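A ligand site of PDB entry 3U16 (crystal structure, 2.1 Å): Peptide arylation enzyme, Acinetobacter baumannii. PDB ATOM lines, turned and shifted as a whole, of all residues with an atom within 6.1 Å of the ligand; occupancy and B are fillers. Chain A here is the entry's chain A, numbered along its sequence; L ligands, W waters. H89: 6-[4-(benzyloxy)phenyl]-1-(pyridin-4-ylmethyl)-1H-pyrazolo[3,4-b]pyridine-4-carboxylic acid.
Merely in contact with the ligand: Leu 239, Pro 240, His 243, Phe 245, Ser 249, Pro 268, Val 288, Gly 316, Val 338, Phe 339 and Ala 342.
Within 4 Å of the ligand: Leu 239, Pro 240, His 243, Asn 244, Phe 245, Ser 249, Pro 268, Val 288, Gly 316, Val 338, Phe 339, Gly 340, Met 341 and Ala 342.
The nearest printed residue that does not touch the ligand is Val 346 (4.01 Å).
N12 of the ligand lies within hydrogen-bond range of N of Gly 340 (2.9 Å).
N6 of the ligand sits at hydrogen-bond distance from ND2 of Asn 244, 3.1 Å away.
The backbone NH (N) of Met 341 sits close to a nitrogen (N6) of the ligand.
Water W1 bridges the backbone carbonyl oxygen of Gly 340 (2.8 Å) and an oxygen (O19) of the ligand (3.4 Å).
ND2 of Asn 244 lies within hydrogen-bond range of O of Met 341 (3.5 Å).
The side-chain hydroxyl (OG) of Ser 248 sits at hydrogen-bond distance from the backbone carbonyl oxygen (O) of Asn 244.
A ring nitrogen (ND1) of His 243 is in hydrogen-bond range of the backbone NH of Phe 245 (3.0 Å).
The side-chain hydroxyl of Ser 249 sits close to the side-chain hydroxyl of Ser 248, at 3.5 Å.
The backbone carbonyl oxygen of Val 314 sits at hydrogen-bond distance from the backbone NH of Val 338 (2.9 Å).
The side-chain sulfur (SD) of Met 246 sits close to the backbone NH (N) of Leu 239.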
ATOM      1  N   ALA A 238      -1.607  -1.698 -27.507  1.00  0.00           N
ATOM      2  CA  ALA A 238      -1.330  -2.444 -26.288  1.00  0.00           C
ATOM      3  C   ALA A 238      -1.999  -3.808 -26.282  1.00  0.00           C
ATOM      4  O   ALA A 238      -1.635  -4.654 -25.474  1.00  0.00           O
ATOM      5  CB  ALA A 238      -1.781  -1.633 -25.031  1.00  0.00           C
ATOM      6  N   LEU A 239      -3.000  -4.027 -27.132  1.00  0.00           N
ATOM      7  CA  LEU A 239      -3.555  -5.369 -27.330  1.00  0.00           C
ATOM      8  C   LEU A 239      -2.658  -6.110 -28.318  1.00  0.00           C
ATOM      9  O   LEU A 239      -1.829  -5.492 -28.961  1.00  0.00           O
ATOM     10  CB  LEU A 239      -5.002  -5.295 -27.841  1.00  0.00           C
ATOM     11  CG  LEU A 239      -6.014  -4.595 -26.923  1.00  0.00           C
ATOM     12  CD1 LEU A 239      -7.380  -4.482 -27.583  1.00  0.00           C
ATOM     13  CD2 LEU A 239      -6.136  -5.340 -25.600  1.00  0.00           C
ATOM     14  N   PRO A 240      -2.800  -7.443 -28.415  1.00  0.00           N
ATOM     15  CA  PRO A 240      -1.951  -8.170 -29.371  1.00  0.00           C
ATOM     16  C   PRO A 240      -2.099  -7.614 -30.800  1.00  0.00           C
ATOM     17  O   PRO A 240      -3.210  -7.516 -31.315  1.00  0.00           O
ATOM     18  CB  PRO A 240      -2.496  -9.603 -29.303  1.00  0.00           C
ATOM     19  CG  PRO A 240      -3.065  -9.708 -27.908  1.00  0.00           C
ATOM     20  CD  PRO A 240      -3.665  -8.356 -27.634  1.00  0.00           C
ATOM     21  N   HIS A 243      -4.397  -9.328 -33.445  1.00  0.00           N
ATOM     22  CA  HIS A 243      -5.836  -9.430 -33.223  1.00  0.00           C
ATOM     23  C   HIS A 243      -6.630  -8.484 -34.136  1.00  0.00           C
ATOM     24  O   HIS A 243      -6.269  -7.317 -34.315  1.00  0.00           O
ATOM     25  CB  HIS A 243      -6.188  -9.184 -31.753  1.00  0.00           C
ATOM     26  CG  HIS A 243      -7.558  -9.655 -31.396  1.00  0.00           C
ATOM     27  ND1 HIS A 243      -8.697  -8.969 -31.778  1.00  0.00           N
ATOM     28  CD2 HIS A 243      -7.982 -10.755 -30.731  1.00  0.00           C
ATOM     29  CE1 HIS A 243      -9.760  -9.632 -31.346  1.00  0.00           C
ATOM     30  NE2 HIS A 243      -9.356 -10.721 -30.723  1.00  0.00           N
ATOM     31  N   ASN A 244      -7.710  -9.001 -34.713  1.00  0.00           N
ATOM     32  CA  ASN A 244      -8.548  -8.224 -35.622  1.00  0.00           C
ATOM     33  C   ASN A 244      -8.874  -6.828 -35.068  1.00  0.00           C
ATOM     34  O   ASN A 244      -8.874  -5.840 -35.794  1.00  0.00           O
ATOM     35  CB  ASN A 244      -9.851  -8.970 -35.932  1.00  0.00           C
ATOM     36  CG  ASN A 244     -10.459  -8.566 -37.286  1.00  0.00           C
ATOM     37  OD1 ASN A 244      -9.791  -8.625 -38.318  1.00  0.00           O
ATOM     38  ND2 ASN A 244     -11.715  -8.149 -37.260  1.00  0.00           N
ATOM     39  N   PHE A 245      -9.137  -6.766 -33.764  1.00  0.00           N
ATOM     40  CA  PHE A 245      -9.518  -5.528 -33.096  1.00  0.00           C
ATOM     41  C   PHE A 245      -8.374  -4.538 -33.231  1.00  0.00           C
ATOM     42  O   PHE A 245      -8.565  -3.409 -33.697  1.00  0.00           O
ATOM     43  CB  PHE A 245      -9.882  -5.830 -31.624  1.00  0.00           C
ATOM     44  CG  PHE A 245     -10.400  -4.630 -30.838  1.00  0.00           C
ATOM     45  CD1 PHE A 245     -10.862  -3.490 -31.472  1.00  0.00           C
ATOM     46  CD2 PHE A 245     -10.434  -4.680 -29.443  1.00  0.00           C
ATOM     47  CE1 PHE A 245     -11.345  -2.397 -30.729  1.00  0.00           C
ATOM     48  CE2 PHE A 245     -10.924  -3.609 -28.692  1.00  0.00           C
ATOM     49  CZ  PHE A 245     -11.377  -2.456 -29.334  1.00  0.00           C
ATOM     50  N   MET A 246      -7.181  -4.983 -32.862  1.00  0.00           N
ATOM     51  CA  MET A 246      -6.000  -4.114 -32.859  1.00  0.00           C
ATOM     52  C   MET A 246      -5.368  -3.907 -34.243  1.00  0.00           C
ATOM     53  O   MET A 246      -4.563  -2.974 -34.446  1.00  0.00           O
ATOM     54  CB  MET A 246      -4.923  -4.690 -31.920  1.00  0.00           C
ATOM     55  CG  MET A 246      -3.853  -3.703 -31.500  1.00  0.00           C
ATOM     56  SD  MET A 246      -4.512  -2.542 -30.271  1.00  0.00           S
ATOM     57  CE  MET A 246      -4.698  -1.044 -31.245  1.00  0.00           C
ATOM     58  N   SER A 248      -7.282  -3.893 -37.330  1.00  0.00           N
ATOM     59  CA  SER A 248      -8.160  -3.359 -38.366  1.00  0.00           C
ATOM     60  C   SER A 248      -9.405  -2.601 -37.894  1.00  0.00           C
ATOM     61  O   SER A 248     -10.175  -2.134 -38.718  1.00  0.00           O
ATOM     62  CB  SER A 248      -8.605  -4.476 -39.318  1.00  0.00           C
ATOM     63  OG  SER A 248      -9.565  -5.319 -38.706  1.00  0.00           O
ATOM     64  N   SER A 249      -9.588  -2.465 -36.587  1.00  0.00           N
ATOM     65  CA  SER A 249     -10.881  -1.997 -36.090  1.00  0.00           C
ATOM     66  C   SER A 249     -10.880  -0.780 -35.165  1.00  0.00           C
ATOM     67  O   SER A 249     -11.477  -0.839 -34.079  1.00  0.00           O
ATOM     68  CB  SER A 249     -11.653  -3.152 -35.434  1.00  0.00           C
ATOM     69  OG  SER A 249     -11.912  -4.179 -36.415  1.00  0.00           O
ATOM     70  N   ASN A 267       2.016  -4.564 -23.643  1.00  0.00           N
ATOM     71  CA  ASN A 267       0.741  -5.035 -23.117  1.00  0.00           C
ATOM     72  C   ASN A 267       0.024  -3.851 -22.476  1.00  0.00           C
ATOM     73  O   ASN A 267       0.544  -2.735 -22.516  1.00  0.00           O
ATOM     74  CB  ASN A 267       0.949  -6.152 -22.101  1.00  0.00           C
ATOM     75  CG  ASN A 267       1.859  -5.735 -20.964  1.00  0.00           C
ATOM     76  OD1 ASN A 267       1.588  -4.772 -20.255  1.00  0.00           O
ATOM     77  ND2 ASN A 267       2.960  -6.455 -20.812  1.00  0.00           N
ATOM     78  N   PRO A 268      -1.166  -4.083 -21.897  1.00  0.00           N
ATOM     79  CA  PRO A 268      -1.914  -2.948 -21.332  1.00  0.00           C
ATOM     80  C   PRO A 268      -1.561  -2.589 -19.884  1.00  0.00           C
ATOM     81  O   PRO A 268      -2.351  -1.884 -19.253  1.00  0.00           O
ATOM     82  CB  PRO A 268      -3.388  -3.410 -21.399  1.00  0.00           C
ATOM     83  CG  PRO A 268      -3.392  -4.674 -22.193  1.00  0.00           C
ATOM     84  CD  PRO A 268      -2.028  -5.279 -22.007  1.00  0.00           C
ATOM     85  N   VAL A 288      -9.752  -3.981 -23.974  1.00  0.00           N
ATOM     86  CA  VAL A 288     -10.848  -4.831 -23.528  1.00  0.00           C
ATOM     87  C   VAL A 288     -11.208  -4.464 -22.070  1.00  0.00           C
ATOM     88  O   VAL A 288     -10.375  -3.911 -21.342  1.00  0.00           O
ATOM     89  CB  VAL A 288     -10.474  -6.304 -23.627  1.00  0.00           C
ATOM     90  CG1 VAL A 288     -10.086  -6.656 -25.080  1.00  0.00           C
ATOM     91  CG2 VAL A 288      -9.318  -6.633 -22.666  1.00  0.00           C
ATOM     92  N   SER A 290     -11.374  -5.847 -19.015  1.00  0.00           N
ATOM     93  CA  SER A 290     -10.466  -6.150 -17.894  1.00  0.00           C
ATOM     94  C   SER A 290      -9.295  -5.169 -17.822  1.00  0.00           C
ATOM     95  O   SER A 290      -8.815  -4.843 -16.728  1.00  0.00           O
ATOM     96  CB  SER A 290      -9.904  -7.583 -17.982  1.00  0.00           C
ATOM     97  OG  SER A 290      -9.174  -7.770 -19.195  1.00  0.00           O
ATOM     98  N   ALA A 291      -8.827  -4.707 -18.972  1.00  0.00           N
ATOM     99  CA  ALA A 291      -7.734  -3.753 -19.015  1.00  0.00           C
ATOM    100  C   ALA A 291      -8.229  -2.332 -18.703  1.00  0.00           C
ATOM    101  O   ALA A 291      -7.521  -1.569 -18.049  1.00  0.00           O
ATOM    102  CB  ALA A 291      -7.004  -3.803 -20.361  1.00  0.00           C
ATOM    103  N   VAL A 314     -13.485   0.406 -26.680  1.00  0.00           N
ATOM    104  CA  VAL A 314     -13.585  -0.725 -25.776  1.00  0.00           C
ATOM    105  C   VAL A 314     -14.430  -1.804 -26.401  1.00  0.00           C
ATOM    106  O   VAL A 314     -15.572  -1.565 -26.811  1.00  0.00           O
ATOM    107  CB  VAL A 314     -14.171  -0.346 -24.388  1.00  0.00           C
ATOM    108  CG1 VAL A 314     -14.216  -1.559 -23.485  1.00  0.00           C
ATOM    109  CG2 VAL A 314     -13.366   0.787 -23.760  1.00  0.00           C
ATOM    110  N   GLY A 315     -13.864  -2.993 -26.510  1.00  0.00           N
ATOM    111  CA  GLY A 315     -14.603  -4.123 -27.045  1.00  0.00           C
ATOM    112  C   GLY A 315     -14.212  -5.351 -26.270  1.00  0.00           C
ATOM    113  O   GLY A 315     -13.162  -5.404 -25.624  1.00  0.00           O
ATOM    114  N   GLY A 316     -15.070  -6.363 -26.340  1.00  0.00           N
ATOM    115  CA  GLY A 316     -14.717  -7.645 -25.774  1.00  0.00           C
ATOM    116  C   GLY A 316     -15.890  -8.214 -25.028  1.00  0.00           C
ATOM    117  O   GLY A 316     -17.001  -8.329 -25.572  1.00  0.00           O
ATOM    118  N   ALA A 317     -15.622  -8.564 -23.782  1.00  0.00           N
ATOM    119  CA  ALA A 317     -16.581  -9.091 -22.827  1.00  0.00           C
ATOM    120  C   ALA A 317     -17.605  -8.046 -22.420  1.00  0.00           C
ATOM    121  O   ALA A 317     -17.704  -6.967 -23.012  1.00  0.00           O
ATOM    122  CB  ALA A 317     -15.820  -9.556 -21.588  1.00  0.00           C
ATOM    123  N   VAL A 338     -17.128  -1.125 -29.210  1.00  0.00           N
ATOM    124  CA  VAL A 338     -16.937  -1.896 -30.431  1.00  0.00           C
ATOM    125  C   VAL A 338     -17.293  -3.353 -30.178  1.00  0.00           C
ATOM    126  O   VAL A 338     -16.795  -3.971 -29.237  1.00  0.00           O
ATOM    127  CB  VAL A 338     -15.467  -1.848 -30.900  1.00  0.00           C
ATOM    128  CG1 VAL A 338     -15.323  -2.540 -32.281  1.00  0.00           C
ATOM    129  CG2 VAL A 338     -14.970  -0.421 -30.925  1.00  0.00           C
ATOM    130  N   PHE A 339     -18.133  -3.912 -31.038  1.00  0.00           N
ATOM    131  CA  PHE A 339     -18.409  -5.333 -30.985  1.00  0.00           C
ATOM    132  C   PHE A 339     -18.169  -5.928 -32.361  1.00  0.00           C
ATOM    133  O   PHE A 339     -18.869  -5.617 -33.325  1.00  0.00           O
ATOM    134  CB  PHE A 339     -19.823  -5.614 -30.495  1.00  0.00           C
ATOM    135  CG  PHE A 339     -20.314  -6.982 -30.864  1.00  0.00           C
ATOM    136  CD1 PHE A 339     -19.744  -8.097 -30.283  1.00  0.00           C
ATOM    137  CD2 PHE A 339     -21.298  -7.142 -31.813  1.00  0.00           C
ATOM    138  CE1 PHE A 339     -20.172  -9.364 -30.643  1.00  0.00           C
ATOM    139  CE2 PHE A 339     -21.726  -8.408 -32.172  1.00  0.00           C
ATOM    140  CZ  PHE A 339     -21.169  -9.515 -31.583  1.00  0.00           C
ATOM    141  N   GLY A 340     -17.138  -6.760 -32.474  1.00  0.00           N
ATOM    142  CA  GLY A 340     -16.750  -7.268 -33.774  1.00  0.00           C
ATOM    143  C   GLY A 340     -16.342  -8.731 -33.715  1.00  0.00           C
ATOM    144  O   GLY A 340     -16.493  -9.379 -32.682  1.00  0.00           O
ATOM    145  N   MET A 341     -15.831  -9.244 -34.832  1.00  0.00           N
ATOM    146  CA  MET A 341     -15.396 -10.635 -34.881  1.00  0.00           C
ATOM    147  C   MET A 341     -14.397 -10.787 -36.017  1.00  0.00           C
ATOM    148  O   MET A 341     -14.552 -10.148 -37.062  1.00  0.00           O
ATOM    149  CB  MET A 341     -16.596 -11.574 -35.070  1.00  0.00           C
ATOM    150  CG  MET A 341     -17.422 -11.282 -36.298  1.00  0.00           C
ATOM    151  SD  MET A 341     -19.059 -12.083 -36.350  1.00  0.00           S
ATOM    152  CE  MET A 341     -19.894 -11.160 -35.058  1.00  0.00           C
ATOM    153  N   ALA A 342     -13.363 -11.587 -35.815  1.00  0.00           N
ATOM    154  CA  ALA A 342     -12.364 -11.827 -36.861  1.00  0.00           C
ATOM    155  C   ALA A 342     -12.997 -12.397 -38.142  1.00  0.00           C
ATOM    156  O   ALA A 342     -12.417 -12.300 -39.231  1.00  0.00           O
ATOM    157  CB  ALA A 342     -11.251 -12.735 -36.350  1.00  0.00           C
ATOM    158  N   GLY A 344     -15.516 -11.189 -39.625  1.00  0.00           N
ATOM    159  CA  GLY A 344     -16.022 -10.092 -40.439  1.00  0.00           C
ATOM    160  C   GLY A 344     -16.698  -8.949 -39.699  1.00  0.00           C
ATOM    161  O   GLY A 344     -16.039  -8.027 -39.217  1.00  0.00           O
ATOM    162  N   LEU A 345     -18.029  -9.018 -39.602  1.00  0.00           N
ATOM    163  CA  LEU A 345     -18.857  -7.956 -39.030  1.00  0.00           C
ATOM    164  C   LEU A 345     -18.225  -7.227 -37.841  1.00  0.00           C
ATOM    165  O   LEU A 345     -17.883  -7.847 -36.825  1.00  0.00           O
ATOM    166  CB  LEU A 345     -20.215  -8.534 -38.579  1.00  0.00           C
ATOM    167  CG  LEU A 345     -21.122  -7.540 -37.847  1.00  0.00           C
ATOM    168  CD1 LEU A 345     -21.557  -6.457 -38.821  1.00  0.00           C
ATOM    169  CD2 LEU A 345     -22.366  -8.194 -37.203  1.00  0.00           C
ATOM    170  N   VAL A 346     -18.102  -5.914 -37.970  1.00  0.00           N
ATOM    171  CA  VAL A 346     -17.715  -5.074 -36.834  1.00  0.00           C
ATOM    172  C   VAL A 346     -18.746  -3.976 -36.621  1.00  0.00           C
ATOM    173  O   VAL A 346     -19.236  -3.378 -37.591  1.00  0.00           O
ATOM    174  CB  VAL A 346     -16.339  -4.405 -37.059  1.00  0.00           C
ATOM    175  CG1 VAL A 346     -15.967  -3.554 -35.844  1.00  0.00           C
ATOM    176  CG2 VAL A 346     -15.262  -5.458 -37.345  1.00  0.00           C
ATOM    177  N   ASP A 422     -23.573 -15.279 -31.217  1.00  0.00           N
ATOM    178  CA  ASP A 422     -23.810 -14.181 -30.291  1.00  0.00           C
ATOM    179  C   ASP A 422     -25.301 -13.948 -30.091  1.00  0.00           C
ATOM    180  O   ASP A 422     -26.087 -14.075 -31.026  1.00  0.00           O
ATOM    181  CB  ASP A 422     -23.154 -12.908 -30.795  1.00  0.00           C
ATOM    182  CG  ASP A 422     -21.662 -13.037 -30.925  1.00  0.00           C
ATOM    183  OD1 ASP A 422     -21.135 -12.950 -32.053  1.00  0.00           O
ATOM    184  OD2 ASP A 422     -21.010 -13.253 -29.889  1.00  0.00           O
HETATM  185  C1  H89 L   1     -12.899  -6.393 -34.247  1.00  0.00           C
HETATM  186  C2  H89 L   1     -13.265  -5.812 -33.025  1.00  0.00           C
HETATM  187  C3  H89 L   1     -13.501  -6.634 -31.924  1.00  0.00           C
HETATM  188  C4  H89 L   1     -13.386  -8.010 -32.098  1.00  0.00           C
HETATM  189  C5  H89 L   1     -13.015  -8.539 -33.340  1.00  0.00           C
HETATM  190  N6  H89 L   1     -12.788  -7.727 -34.382  1.00  0.00           N
HETATM  191  C7  H89 L   1     -13.908  -6.076 -30.556  1.00  0.00           C
HETATM  192  N8  H89 L   1     -14.399  -7.255 -29.841  1.00  0.00           N
HETATM  193  C9  H89 L   1     -13.764  -8.162 -29.118  1.00  0.00           C
HETATM  194  C10 H89 L   1     -14.730  -9.076 -28.771  1.00  0.00           C
HETATM  195  C11 H89 L   1     -16.005  -8.701 -29.316  1.00  0.00           C
HETATM  196  N12 H89 L   1     -15.763  -7.550 -29.992  1.00  0.00           N
HETATM  197  N13 H89 L   1     -12.471  -8.287 -28.744  1.00  0.00           N
HETATM  198  C14 H89 L   1     -12.090  -9.315 -27.983  1.00  0.00           C
HETATM  199  C15 H89 L   1     -13.015 -10.281 -27.587  1.00  0.00           C
HETATM  200  C16 H89 L   1     -14.345 -10.163 -27.978  1.00  0.00           C
HETATM  201  C18 H89 L   1     -15.335 -11.209 -27.542  1.00  0.00           C
HETATM  202  O19 H89 L   1     -16.546 -11.131 -27.871  1.00  0.00           O
HETATM  203  O20 H89 L   1     -14.928 -12.153 -26.837  1.00  0.00           O
HETATM  204  C21 H89 L   1     -10.657  -9.407 -27.616  1.00  0.00           C
HETATM  205  C22 H89 L   1      -9.764  -8.618 -28.320  1.00  0.00           C
HETATM  206  C23 H89 L   1      -8.408  -8.665 -28.027  1.00  0.00           C
HETATM  207  C24 H89 L   1      -7.948  -9.499 -27.020  1.00  0.00           C
HETATM  208  C25 H89 L   1      -8.854 -10.289 -26.297  1.00  0.00           C
HETATM  209  C26 H89 L   1     -10.216 -10.254 -26.601  1.00  0.00           C
HETATM  210  O27 H89 L   1      -6.611  -9.539 -26.740  1.00  0.00           O
HETATM  211  C28 H89 L   1      -5.605  -9.617 -24.539  1.00  0.00           C
HETATM  212  C29 H89 L   1      -6.275  -8.793 -23.644  1.00  0.00           C
HETATM  213  C30 H89 L   1      -5.569  -8.099 -22.665  1.00  0.00           C
HETATM  214  C31 H89 L   1      -4.182  -8.239 -22.590  1.00  0.00           C
HETATM  215  C32 H89 L   1      -3.493  -9.060 -23.481  1.00  0.00           C
HETATM  216  C33 H89 L   1      -4.219  -9.757 -24.453  1.00  0.00           C
HETATM  217  C34 H89 L   1      -6.378 -10.375 -25.600  1.00  0.00           C
HETATM  218  O   HOH W   1     -16.593 -11.728 -31.243  1.00  0.00           O
